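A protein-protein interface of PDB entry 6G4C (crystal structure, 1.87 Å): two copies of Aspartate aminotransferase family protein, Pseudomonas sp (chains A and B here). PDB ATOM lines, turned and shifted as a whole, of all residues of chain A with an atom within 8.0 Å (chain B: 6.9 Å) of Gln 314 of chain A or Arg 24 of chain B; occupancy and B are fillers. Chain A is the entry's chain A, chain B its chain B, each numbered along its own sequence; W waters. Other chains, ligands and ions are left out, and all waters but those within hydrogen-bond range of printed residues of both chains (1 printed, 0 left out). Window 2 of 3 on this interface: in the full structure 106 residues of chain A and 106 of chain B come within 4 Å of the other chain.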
ATOM      1  N   HIS A  88     -11.734  15.253 -19.672  1.00  0.00           N
ATOM      2  CA  HIS A  88     -11.214  14.264 -18.719  1.00  0.00           C
ATOM      3  C   HIS A  88     -11.693  14.415 -17.284  1.00  0.00           C
ATOM      4  O   HIS A  88     -11.379  13.530 -16.450  1.00  0.00           O
ATOM      5  CB  HIS A  88      -9.673  14.189 -18.713  1.00  0.00           C
ATOM      6  CG  HIS A  88      -9.057  14.050 -20.069  1.00  0.00           C
ATOM      7  ND1 HIS A  88      -8.967  12.845 -20.726  1.00  0.00           N
ATOM      8  CD2 HIS A  88      -8.455  14.959 -20.872  1.00  0.00           C
ATOM      9  CE1 HIS A  88      -8.372  13.017 -21.891  1.00  0.00           C
ATOM     10  NE2 HIS A  88      -8.048  14.292 -22.005  1.00  0.00           N
ATOM     11  N   LYS A 111     -19.913   1.404 -23.356  1.00  0.00           N
ATOM     12  CA  LYS A 111     -19.819   2.734 -22.743  1.00  0.00           C
ATOM     13  C   LYS A 111     -21.196   3.372 -22.531  1.00  0.00           C
ATOM     14  O   LYS A 111     -22.156   3.023 -23.232  1.00  0.00           O
ATOM     15  CB  LYS A 111     -18.990   3.662 -23.632  1.00  0.00           C
ATOM     16  CG  LYS A 111     -17.550   3.213 -23.879  1.00  0.00           C
ATOM     17  CD  LYS A 111     -16.680   3.315 -22.644  1.00  0.00           C
ATOM     18  CE  LYS A 111     -15.306   2.641 -22.859  1.00  0.00           C
ATOM     19  NZ  LYS A 111     -15.426   1.146 -22.841  1.00  0.00           N
ATOM     20  N   TYR A 131     -21.277  10.331 -37.145  1.00  0.00           N
ATOM     21  CA  TYR A 131     -19.854  10.426 -36.803  1.00  0.00           C
ATOM     22  C   TYR A 131     -19.154   9.098 -37.012  1.00  0.00           C
ATOM     23  O   TYR A 131     -18.099   9.040 -37.641  1.00  0.00           O
ATOM     24  CB  TYR A 131     -19.761  10.859 -35.343  1.00  0.00           C
ATOM     25  CG  TYR A 131     -18.447  11.345 -34.794  1.00  0.00           C
ATOM     26  CD1 TYR A 131     -18.060  12.671 -34.954  1.00  0.00           C
ATOM     27  CD2 TYR A 131     -17.670  10.527 -33.984  1.00  0.00           C
ATOM     28  CE1 TYR A 131     -16.913  13.164 -34.363  1.00  0.00           C
ATOM     29  CE2 TYR A 131     -16.522  11.015 -33.374  1.00  0.00           C
ATOM     30  CZ  TYR A 131     -16.150  12.342 -33.578  1.00  0.00           C
ATOM     31  OH  TYR A 131     -15.004  12.838 -32.988  1.00  0.00           O
ATOM     32  N   ALA A 303     -19.575  -2.303 -28.280  1.00  0.00           N
ATOM     33  CA  ALA A 303     -18.140  -2.176 -28.573  1.00  0.00           C
ATOM     34  C   ALA A 303     -17.811  -1.599 -29.970  1.00  0.00           C
ATOM     35  O   ALA A 303     -17.055  -0.649 -30.061  1.00  0.00           O
ATOM     36  CB  ALA A 303     -17.429  -3.520 -28.353  1.00  0.00           C
ATOM     37  N   PRO A 304     -18.382  -2.154 -31.047  1.00  0.00           N
ATOM     38  CA  PRO A 304     -18.110  -1.595 -32.387  1.00  0.00           C
ATOM     39  C   PRO A 304     -18.465  -0.111 -32.530  1.00  0.00           C
ATOM     40  O   PRO A 304     -17.702   0.669 -33.114  1.00  0.00           O
ATOM     41  CB  PRO A 304     -18.984  -2.415 -33.323  1.00  0.00           C
ATOM     42  CG  PRO A 304     -19.429  -3.594 -32.550  1.00  0.00           C
ATOM     43  CD  PRO A 304     -19.218  -3.359 -31.092  1.00  0.00           C
ATOM     44  N   PHE A 306     -18.546   2.146 -30.045  1.00  0.00           N
ATOM     45  CA  PHE A 306     -17.547   2.879 -29.274  1.00  0.00           C
ATOM     46  C   PHE A 306     -16.204   2.952 -30.007  1.00  0.00           C
ATOM     47  O   PHE A 306     -15.607   4.018 -30.103  1.00  0.00           O
ATOM     48  CB  PHE A 306     -17.311   2.271 -27.892  1.00  0.00           C
ATOM     49  CG  PHE A 306     -16.072   2.817 -27.216  1.00  0.00           C
ATOM     50  CD1 PHE A 306     -16.004   4.156 -26.855  1.00  0.00           C
ATOM     51  CD2 PHE A 306     -14.963   2.014 -27.008  1.00  0.00           C
ATOM     52  CE1 PHE A 306     -14.852   4.677 -26.271  1.00  0.00           C
ATOM     53  CE2 PHE A 306     -13.809   2.528 -26.418  1.00  0.00           C
ATOM     54  CZ  PHE A 306     -13.758   3.866 -26.043  1.00  0.00           C
ATOM     55  N   GLU A 307     -15.749   1.827 -30.536  1.00  0.00           N
ATOM     56  CA  GLU A 307     -14.417   1.809 -31.124  1.00  0.00           C
ATOM     57  C   GLU A 307     -14.307   2.786 -32.311  1.00  0.00           C
ATOM     58  O   GLU A 307     -13.311   3.521 -32.422  1.00  0.00           O
ATOM     59  CB  GLU A 307     -14.012   0.393 -31.532  1.00  0.00           C
ATOM     60  CG  GLU A 307     -13.884  -0.587 -30.370  1.00  0.00           C
ATOM     61  CD  GLU A 307     -12.790  -0.218 -29.361  1.00  0.00           C
ATOM     62  OE1 GLU A 307     -11.834   0.518 -29.699  1.00  0.00           O
ATOM     63  OE2 GLU A 307     -12.895  -0.683 -28.209  1.00  0.00           O
ATOM     64  N   GLY A 308     -15.322   2.827 -33.174  1.00  0.00           N
ATOM     65  CA  GLY A 308     -15.309   3.767 -34.321  1.00  0.00           C
ATOM     66  C   GLY A 308     -15.347   5.232 -33.887  1.00  0.00           C
ATOM     67  O   GLY A 308     -14.589   6.075 -34.391  1.00  0.00           O
ATOM     68  N   ILE A 309     -16.224   5.543 -32.942  1.00  0.00           N
ATOM     69  CA  ILE A 309     -16.272   6.886 -32.358  1.00  0.00           C
ATOM     70  C   ILE A 309     -14.944   7.285 -31.691  1.00  0.00           C
ATOM     71  O   ILE A 309     -14.444   8.406 -31.874  1.00  0.00           O
ATOM     72  CB  ILE A 309     -17.409   6.990 -31.337  1.00  0.00           C
ATOM     73  CG1 ILE A 309     -18.732   6.906 -32.085  1.00  0.00           C
ATOM     74  CG2 ILE A 309     -17.316   8.291 -30.533  1.00  0.00           C
ATOM     75  CD1 ILE A 309     -19.920   6.768 -31.174  1.00  0.00           C
ATOM     76  N   ALA A 310     -14.390   6.370 -30.901  1.00  0.00           N
ATOM     77  CA  ALA A 310     -13.155   6.643 -30.174  1.00  0.00           C
ATOM     78  C   ALA A 310     -12.030   6.984 -31.132  1.00  0.00           C
ATOM     79  O   ALA A 310     -11.282   7.938 -30.920  1.00  0.00           O
ATOM     80  CB  ALA A 310     -12.778   5.438 -29.338  1.00  0.00           C
ATOM     81  N   ASP A 311     -11.942   6.217 -32.215  1.00  0.00           N
ATOM     82  CA  ASP A 311     -10.948   6.468 -33.242  1.00  0.00           C
ATOM     83  C   ASP A 311     -11.070   7.860 -33.852  1.00  0.00           C
ATOM     84  O   ASP A 311     -10.076   8.561 -33.973  1.00  0.00           O
ATOM     85  CB  ASP A 311     -11.033   5.394 -34.329  1.00  0.00           C
ATOM     86  CG  ASP A 311     -10.409   4.087 -33.891  1.00  0.00           C
ATOM     87  OD1 ASP A 311      -9.596   4.096 -32.935  1.00  0.00           O
ATOM     88  OD2 ASP A 311     -10.734   3.046 -34.498  1.00  0.00           O
ATOM     89  N   GLN A 312     -12.282   8.262 -34.218  1.00  0.00           N
ATOM     90  CA  GLN A 312     -12.497   9.577 -34.807  1.00  0.00           C
ATOM     91  C   GLN A 312     -12.238  10.699 -33.802  1.00  0.00           C
ATOM     92  O   GLN A 312     -11.647  11.713 -34.163  1.00  0.00           O
ATOM     93  CB  GLN A 312     -13.921   9.664 -35.362  1.00  0.00           C
ATOM     94  CG  GLN A 312     -14.326  10.916 -36.104  1.00  0.00           C
ATOM     95  CD  GLN A 312     -14.041  10.793 -37.565  1.00  0.00           C
ATOM     96  OE1 GLN A 312     -12.919  10.548 -37.931  1.00  0.00           O
ATOM     97  NE2 GLN A 312     -15.064  10.947 -38.407  1.00  0.00           N
ATOM     98  N   SER A 313     -12.647  10.510 -32.542  1.00  0.00           N
ATOM     99  CA  SER A 313     -12.442  11.540 -31.508  1.00  0.00           C
ATOM    100  C   SER A 313     -10.961  11.851 -31.301  1.00  0.00           C
ATOM    101  O   SER A 313     -10.607  12.977 -30.914  1.00  0.00           O
ATOM    102  CB  SER A 313     -13.071  11.135 -30.176  1.00  0.00           C
ATOM    103  OG  SER A 313     -12.255  10.225 -29.447  1.00  0.00           O
ATOM    104  N   GLN A 314     -10.119  10.850 -31.568  1.00  0.00           N
ATOM    105  CA  GLN A 314      -8.676  11.005 -31.544  1.00  0.00           C
ATOM    106  C   GLN A 314      -8.234  11.827 -32.760  1.00  0.00           C
ATOM    107  O   GLN A 314      -7.628  12.874 -32.610  1.00  0.00           O
ATOM    108  CB  GLN A 314      -8.010   9.621 -31.525  1.00  0.00           C
ATOM    109  CG  GLN A 314      -6.488   9.616 -31.609  1.00  0.00           C
ATOM    110  CD  GLN A 314      -5.897   8.224 -31.512  1.00  0.00           C
ATOM    111  OE1 GLN A 314      -6.208   7.335 -32.319  1.00  0.00           O
ATOM    112  NE2 GLN A 314      -5.024   8.026 -30.543  1.00  0.00           N
ATOM    113  N   ALA A 315      -8.586  11.373 -33.960  1.00  0.00           N
ATOM    114  CA  ALA A 315      -8.245  12.097 -35.215  1.00  0.00           C
ATOM    115  C   ALA A 315      -8.737  13.559 -35.249  1.00  0.00           C
ATOM    116  O   ALA A 315      -8.067  14.435 -35.803  1.00  0.00           O
ATOM    117  CB  ALA A 315      -8.794  11.342 -36.416  1.00  0.00           C
ATOM    118  N   LEU A 316      -9.907  13.807 -34.672  1.00  0.00           N
ATOM    119  CA  LEU A 316     -10.496  15.146 -34.626  1.00  0.00           C
ATOM    120  C   LEU A 316     -10.270  15.903 -33.323  1.00  0.00           C
ATOM    121  O   LEU A 316     -10.911  16.940 -33.091  1.00  0.00           O
ATOM    122  CB  LEU A 316     -11.998  15.078 -34.897  1.00  0.00           C
ATOM    123  CG  LEU A 316     -12.438  14.356 -36.168  1.00  0.00           C
ATOM    124  CD1 LEU A 316     -13.945  14.469 -36.328  1.00  0.00           C
ATOM    125  CD2 LEU A 316     -11.737  14.912 -37.393  1.00  0.00           C
ATOM    126  N   GLY A 317      -9.375  15.417 -32.469  1.00  0.00           N
ATOM    127  CA  GLY A 317      -8.916  16.192 -31.320  1.00  0.00           C
ATOM    128  C   GLY A 317      -9.634  15.834 -30.037  1.00  0.00           C
ATOM    129  O   GLY A 317      -9.005  15.594 -29.005  1.00  0.00           O
ATOM    130  N   ALA A 318     -10.952  15.852 -30.083  1.00  0.00           N
ATOM    131  CA  ALA A 318     -11.791  15.485 -28.941  1.00  0.00           C
ATOM    132  C   ALA A 318     -13.187  15.284 -29.517  1.00  0.00           C
ATOM    133  O   ALA A 318     -13.477  15.772 -30.611  1.00  0.00           O
ATOM    134  CB  ALA A 318     -11.813  16.587 -27.905  1.00  0.00           C
ATOM    135  N   LEU A 319     -14.024  14.547 -28.801  1.00  0.00           N
ATOM    136  CA  LEU A 319     -15.417  14.371 -29.198  1.00  0.00           C
ATOM    137  C   LEU A 319     -16.144  15.702 -28.978  1.00  0.00           C
ATOM    138  O   LEU A 319     -16.337  16.104 -27.841  1.00  0.00           O
ATOM    139  CB  LEU A 319     -16.053  13.262 -28.361  1.00  0.00           C
ATOM    140  CG  LEU A 319     -17.516  12.933 -28.663  1.00  0.00           C
ATOM    141  CD1 LEU A 319     -17.652  12.515 -30.099  1.00  0.00           C
ATOM    142  CD2 LEU A 319     -17.985  11.809 -27.757  1.00  0.00           C
ATOM    143  N   THR B  21     -13.851  15.273 -24.929  1.00  0.00           N
ATOM    144  CA  THR B  21     -12.647  14.539 -24.532  1.00  0.00           C
ATOM    145  C   THR B  21     -12.218  13.648 -25.684  1.00  0.00           C
ATOM    146  O   THR B  21     -13.054  13.123 -26.410  1.00  0.00           O
ATOM    147  CB  THR B  21     -12.928  13.673 -23.286  1.00  0.00           C
ATOM    148  OG1 THR B  21     -13.339  14.525 -22.203  1.00  0.00           O
ATOM    149  CG2 THR B  21     -11.703  12.904 -22.855  1.00  0.00           C
ATOM    150  N   ASN B  22     -10.909  13.575 -25.898  1.00  0.00           N
ATOM    151  CA  ASN B  22     -10.300  12.625 -26.826  1.00  0.00           C
ATOM    152  C   ASN B  22     -10.368  11.263 -26.161  1.00  0.00           C
ATOM    153  O   ASN B  22      -9.707  11.035 -25.133  1.00  0.00           O
ATOM    154  CB  ASN B  22      -8.840  13.039 -27.086  1.00  0.00           C
ATOM    155  CG  ASN B  22      -8.044  12.004 -27.876  1.00  0.00           C
ATOM    156  OD1 ASN B  22      -8.372  10.814 -27.920  1.00  0.00           O
ATOM    157  ND2 ASN B  22      -6.954  12.457 -28.468  1.00  0.00           N
ATOM    158  N   ALA B  23     -11.172  10.367 -26.726  1.00  0.00           N
ATOM    159  CA  ALA B  23     -11.520   9.122 -26.039  1.00  0.00           C
ATOM    160  C   ALA B  23     -10.314   8.188 -25.906  1.00  0.00           C
ATOM    161  O   ALA B  23     -10.204   7.430 -24.917  1.00  0.00           O
ATOM    162  CB  ALA B  23     -12.647   8.413 -26.767  1.00  0.00           C
ATOM    163  N   ARG B  24      -9.434   8.204 -26.910  1.00  0.00           N
ATOM    164  CA  ARG B  24      -8.231   7.344 -26.874  1.00  0.00           C
ATOM    165  C   ARG B  24      -7.265   7.850 -25.823  1.00  0.00           C
ATOM    166  O   ARG B  24      -6.725   7.061 -25.049  1.00  0.00           O
ATOM    167  CB  ARG B  24      -7.545   7.264 -28.247  1.00  0.00           C
ATOM    168  CG  ARG B  24      -8.382   6.554 -29.302  1.00  0.00           C
ATOM    169  CD  ARG B  24      -8.734   5.146 -28.835  1.00  0.00           C
ATOM    170  NE  ARG B  24      -9.318   4.322 -29.883  1.00  0.00           N
ATOM    171  CZ  ARG B  24     -10.004   3.201 -29.673  1.00  0.00           C
ATOM    172  NH1 ARG B  24     -10.204   2.743 -28.440  1.00  0.00           N
ATOM    173  NH2 ARG B  24     -10.517   2.537 -30.707  1.00  0.00           N
ATOM    174  N   LEU B  25      -7.055   9.160 -25.791  1.00  0.00           N
ATOM    175  CA  LEU B  25      -6.183   9.771 -24.795  1.00  0.00           C
ATOM    176  C   LEU B  25      -6.736   9.493 -23.399  1.00  0.00           C
ATOM    177  O   LEU B  25      -5.990   9.229 -22.463  1.00  0.00           O
ATOM    178  CB  LEU B  25      -6.054  11.275 -25.042  1.00  0.00           C
ATOM    179  CG  LEU B  25      -5.124  12.065 -24.109  1.00  0.00           C
ATOM    180  CD1 LEU B  25      -3.713  11.488 -24.151  1.00  0.00           C
ATOM    181  CD2 LEU B  25      -5.128  13.539 -24.494  1.00  0.00           C
ATOM    182  N   HIS B  26      -8.063   9.518 -23.276  1.00  0.00           N
ATOM    183  CA  HIS B  26      -8.702   9.265 -21.996  1.00  0.00           C
ATOM    184  C   HIS B  26      -8.403   7.847 -21.511  1.00  0.00           C
ATOM    185  O   HIS B  26      -8.211   7.624 -20.303  1.00  0.00           O
ATOM    186  CB  HIS B  26     -10.217   9.476 -22.077  1.00  0.00           C
ATOM    187  CG  HIS B  26     -10.873   9.478 -20.740  1.00  0.00           C
ATOM    188  ND1 HIS B  26     -10.720  10.506 -19.840  1.00  0.00           N
ATOM    189  CD2 HIS B  26     -11.636   8.549 -20.120  1.00  0.00           C
ATOM    190  CE1 HIS B  26     -11.364  10.218 -18.721  1.00  0.00           C
ATOM    191  NE2 HIS B  26     -11.942   9.042 -18.870  1.00  0.00           N
ATOM    192  N   GLN B  27      -8.374   6.889 -22.432  1.00  0.00           N
ATOM    193  CA  GLN B  27      -8.045   5.525 -22.052  1.00  0.00           C
ATOM    194  C   GLN B  27      -6.598   5.434 -21.526  1.00  0.00           C
ATOM    195  O   GLN B  27      -6.313   4.613 -20.663  1.00  0.00           O
ATOM    196  CB  GLN B  27      -8.251   4.571 -23.215  1.00  0.00           C
ATOM    197  CG  GLN B  27      -9.703   4.415 -23.647  1.00  0.00           C
ATOM    198  CD  GLN B  27      -9.857   3.438 -24.787  1.00  0.00           C
ATOM    199  OE1 GLN B  27      -9.345   3.669 -25.879  1.00  0.00           O
ATOM    200  NE2 GLN B  27     -10.570   2.352 -24.545  1.00  0.00           N
ATOM    201  N   GLU B  28      -5.695   6.268 -22.039  1.00  0.00           N
ATOM    202  CA  GLU B  28      -4.319   6.272 -21.549  1.00  0.00           C
ATOM    203  C   GLU B  28      -4.180   7.010 -20.226  1.00  0.00           C
ATOM    204  O   GLU B  28      -3.636   6.464 -19.269  1.00  0.00           O
ATOM    205  CB  GLU B  28      -3.353   6.902 -22.547  1.00  0.00           C
ATOM    206  CG  GLU B  28      -1.907   6.759 -22.077  1.00  0.00           C
ATOM    207  CD  GLU B  28      -0.943   7.731 -22.723  1.00  0.00           C
ATOM    208  OE1 GLU B  28      -1.290   8.306 -23.774  1.00  0.00           O
ATOM    209  OE2 GLU B  28       0.170   7.907 -22.173  1.00  0.00           O
ATOM    210  N   LEU B  29      -4.683   8.243 -20.175  1.00  0.00           N
ATOM    211  CA  LEU B  29      -4.499   9.109 -19.006  1.00  0.00           C
ATOM    212  C   LEU B  29      -5.482   8.871 -17.868  1.00  0.00           C
ATOM    213  O   LEU B  29      -5.154   9.120 -16.712  1.00  0.00           O
ATOM    214  CB  LEU B  29      -4.634  10.571 -19.410  1.00  0.00           C
ATOM    215  CG  LEU B  29      -3.660  11.081 -20.456  1.00  0.00           C
ATOM    216  CD1 LEU B  29      -3.931  12.556 -20.691  1.00  0.00           C
ATOM    217  CD2 LEU B  29      -2.224  10.859 -20.011  1.00  0.00           C
HETATM  218  O   HOH W   1      -9.116  15.262 -24.363  1.00  0.00           O
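Water W1 lies within hydrogen-bond range of a ring nitrogen (NE2) of His 88 of chain A (2.8 Å) and the backbone NH (N) of Asn 22 of chain B (2.9 Å).
N of Ser 313 of chain A lies close to OH of Tyr 131 of chain A, at 3.3 Å. OG of Ser 313 of chain A lies within hydrogen-bond range of O of Ala 310 of chain A (2.9 Å). The backbone carbonyl oxygen (O) of Ser 313 of chain A lies within hydrogen-bond range of the backbone NH (N) of Ala 318 of chain A (3.0 Å). The side-chain amide oxygen (OD1) of Asn 22 of chain B lies within hydrogen-bond range of the backbone NH (N) of Arg 24 of chain B, 3.0 Å away. The backbone NH (N) of Leu 25 of chain B sits at hydrogen-bond distance from the side-chain amide oxygen (OD1) of Asn 22 of chain B (3.0 Å). NH1 of Arg 24 of chain B lies within hydrogen-bond range of OE1 of Gln 27 of chain B, 2.9 Å away.
No position is printed for both chains. Of the 16 pairs that touch across the chains among the printed residues, none has its exchanged pair printed and touching as well.
Of the 9 printed residues of chain B, 7 touch a printed residue of chain A. Hydrophobic or aromatic side chains of chain B within 4 Å of the printed part of chain A: Ala 23, Leu 25 and His 26. Of the 19 printed residues of chain A, 10 touch a printed residue of chain B. Among the printed residues, Asp or Glu carboxylates within 4 Å of a Lys or Arg side-chain nitrogen of the other chain: Glu 307 of chain A with Arg 24 of chain B and Asp 311 of chain A with Arg 24 of chain B.
Of the printed residues of chain B, His 88 of chain A touches Thr 21 (3.1 Å), Leu 25 (3.9 Å) and His 26 (3.1 Å). Of the printed residues of chain B, Phe 306 of chain A touches Gln 27. Of the printed residues of chain B, Glu 307 of chain A touches Arg 24 (2.6 Å). Gln 314 of chain A touches just these residues of chain B: Asn 22 and Arg 24. Of the printed residues of chain B, Leu 319 of chain A touches Thr 21 (2.9 Å). Arg 24 of chain B touches just these residues of chain A: Glu 307, Ala 310, Asp 311 and Gln 314. Of the printed residues of chain A, His 26 of chain B touches His 88. The nearest printed residue of chain A that does not touch His 26 of chain B is Lys 111 of chain A (7.5 Å).
The side-chain hydroxyl (OG1) of Thr 21 of chain B lies within hydrogen-bond range of the backbone NH (N) of His 88 of chain A (3.1 Å). ND1 of His 88 of chain A lies within hydrogen-bond range of ND1 of His 26 of chain B (3.1 Å). The side-chain carboxylate (OE1) of Glu 307 of chain A is in salt-bridge range of the guanidinium group (NH2) of Arg 24 of chain B, 2.6 Å away. The side-chain carboxylate (OD1) of Asp 311 of chain A lies within salt-bridge range of the guanidinium group (NH2) of Arg 24 of chain B. The side-chain hydroxyl (OG) of Ser 313 of chain A sits at hydrogen-bond distance from the backbone NH (N) of Ala 23 of chain B (2.9 Å). The backbone NH of Leu 319 of chain A sits at hydrogen-bond distance from the backbone carbonyl oxygen of Thr 21 of chain B, 2.9 Å away.
Among the printed residues, pairs that only touch across the chains: Gly 317 of chain A with Asn 22 of chain B, Gln 314 of chain A with Arg 24 of chain B, Ala 310 of chain A with Arg 24 of chain B, Gln 314 of chain A with Asn 22 of chain B, Ala 318 of chain A with Thr 21 of chain B, Ala 318 of chain A with Asn 22 of chain B, Phe 306 of chain A with Gln 27 of chain B, Ala 310 of chain A with Ala 23 of chain B, His 88 of chain A with Leu 25 of chain B and Ser 313 of chain A with Asn 22 of chain B.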
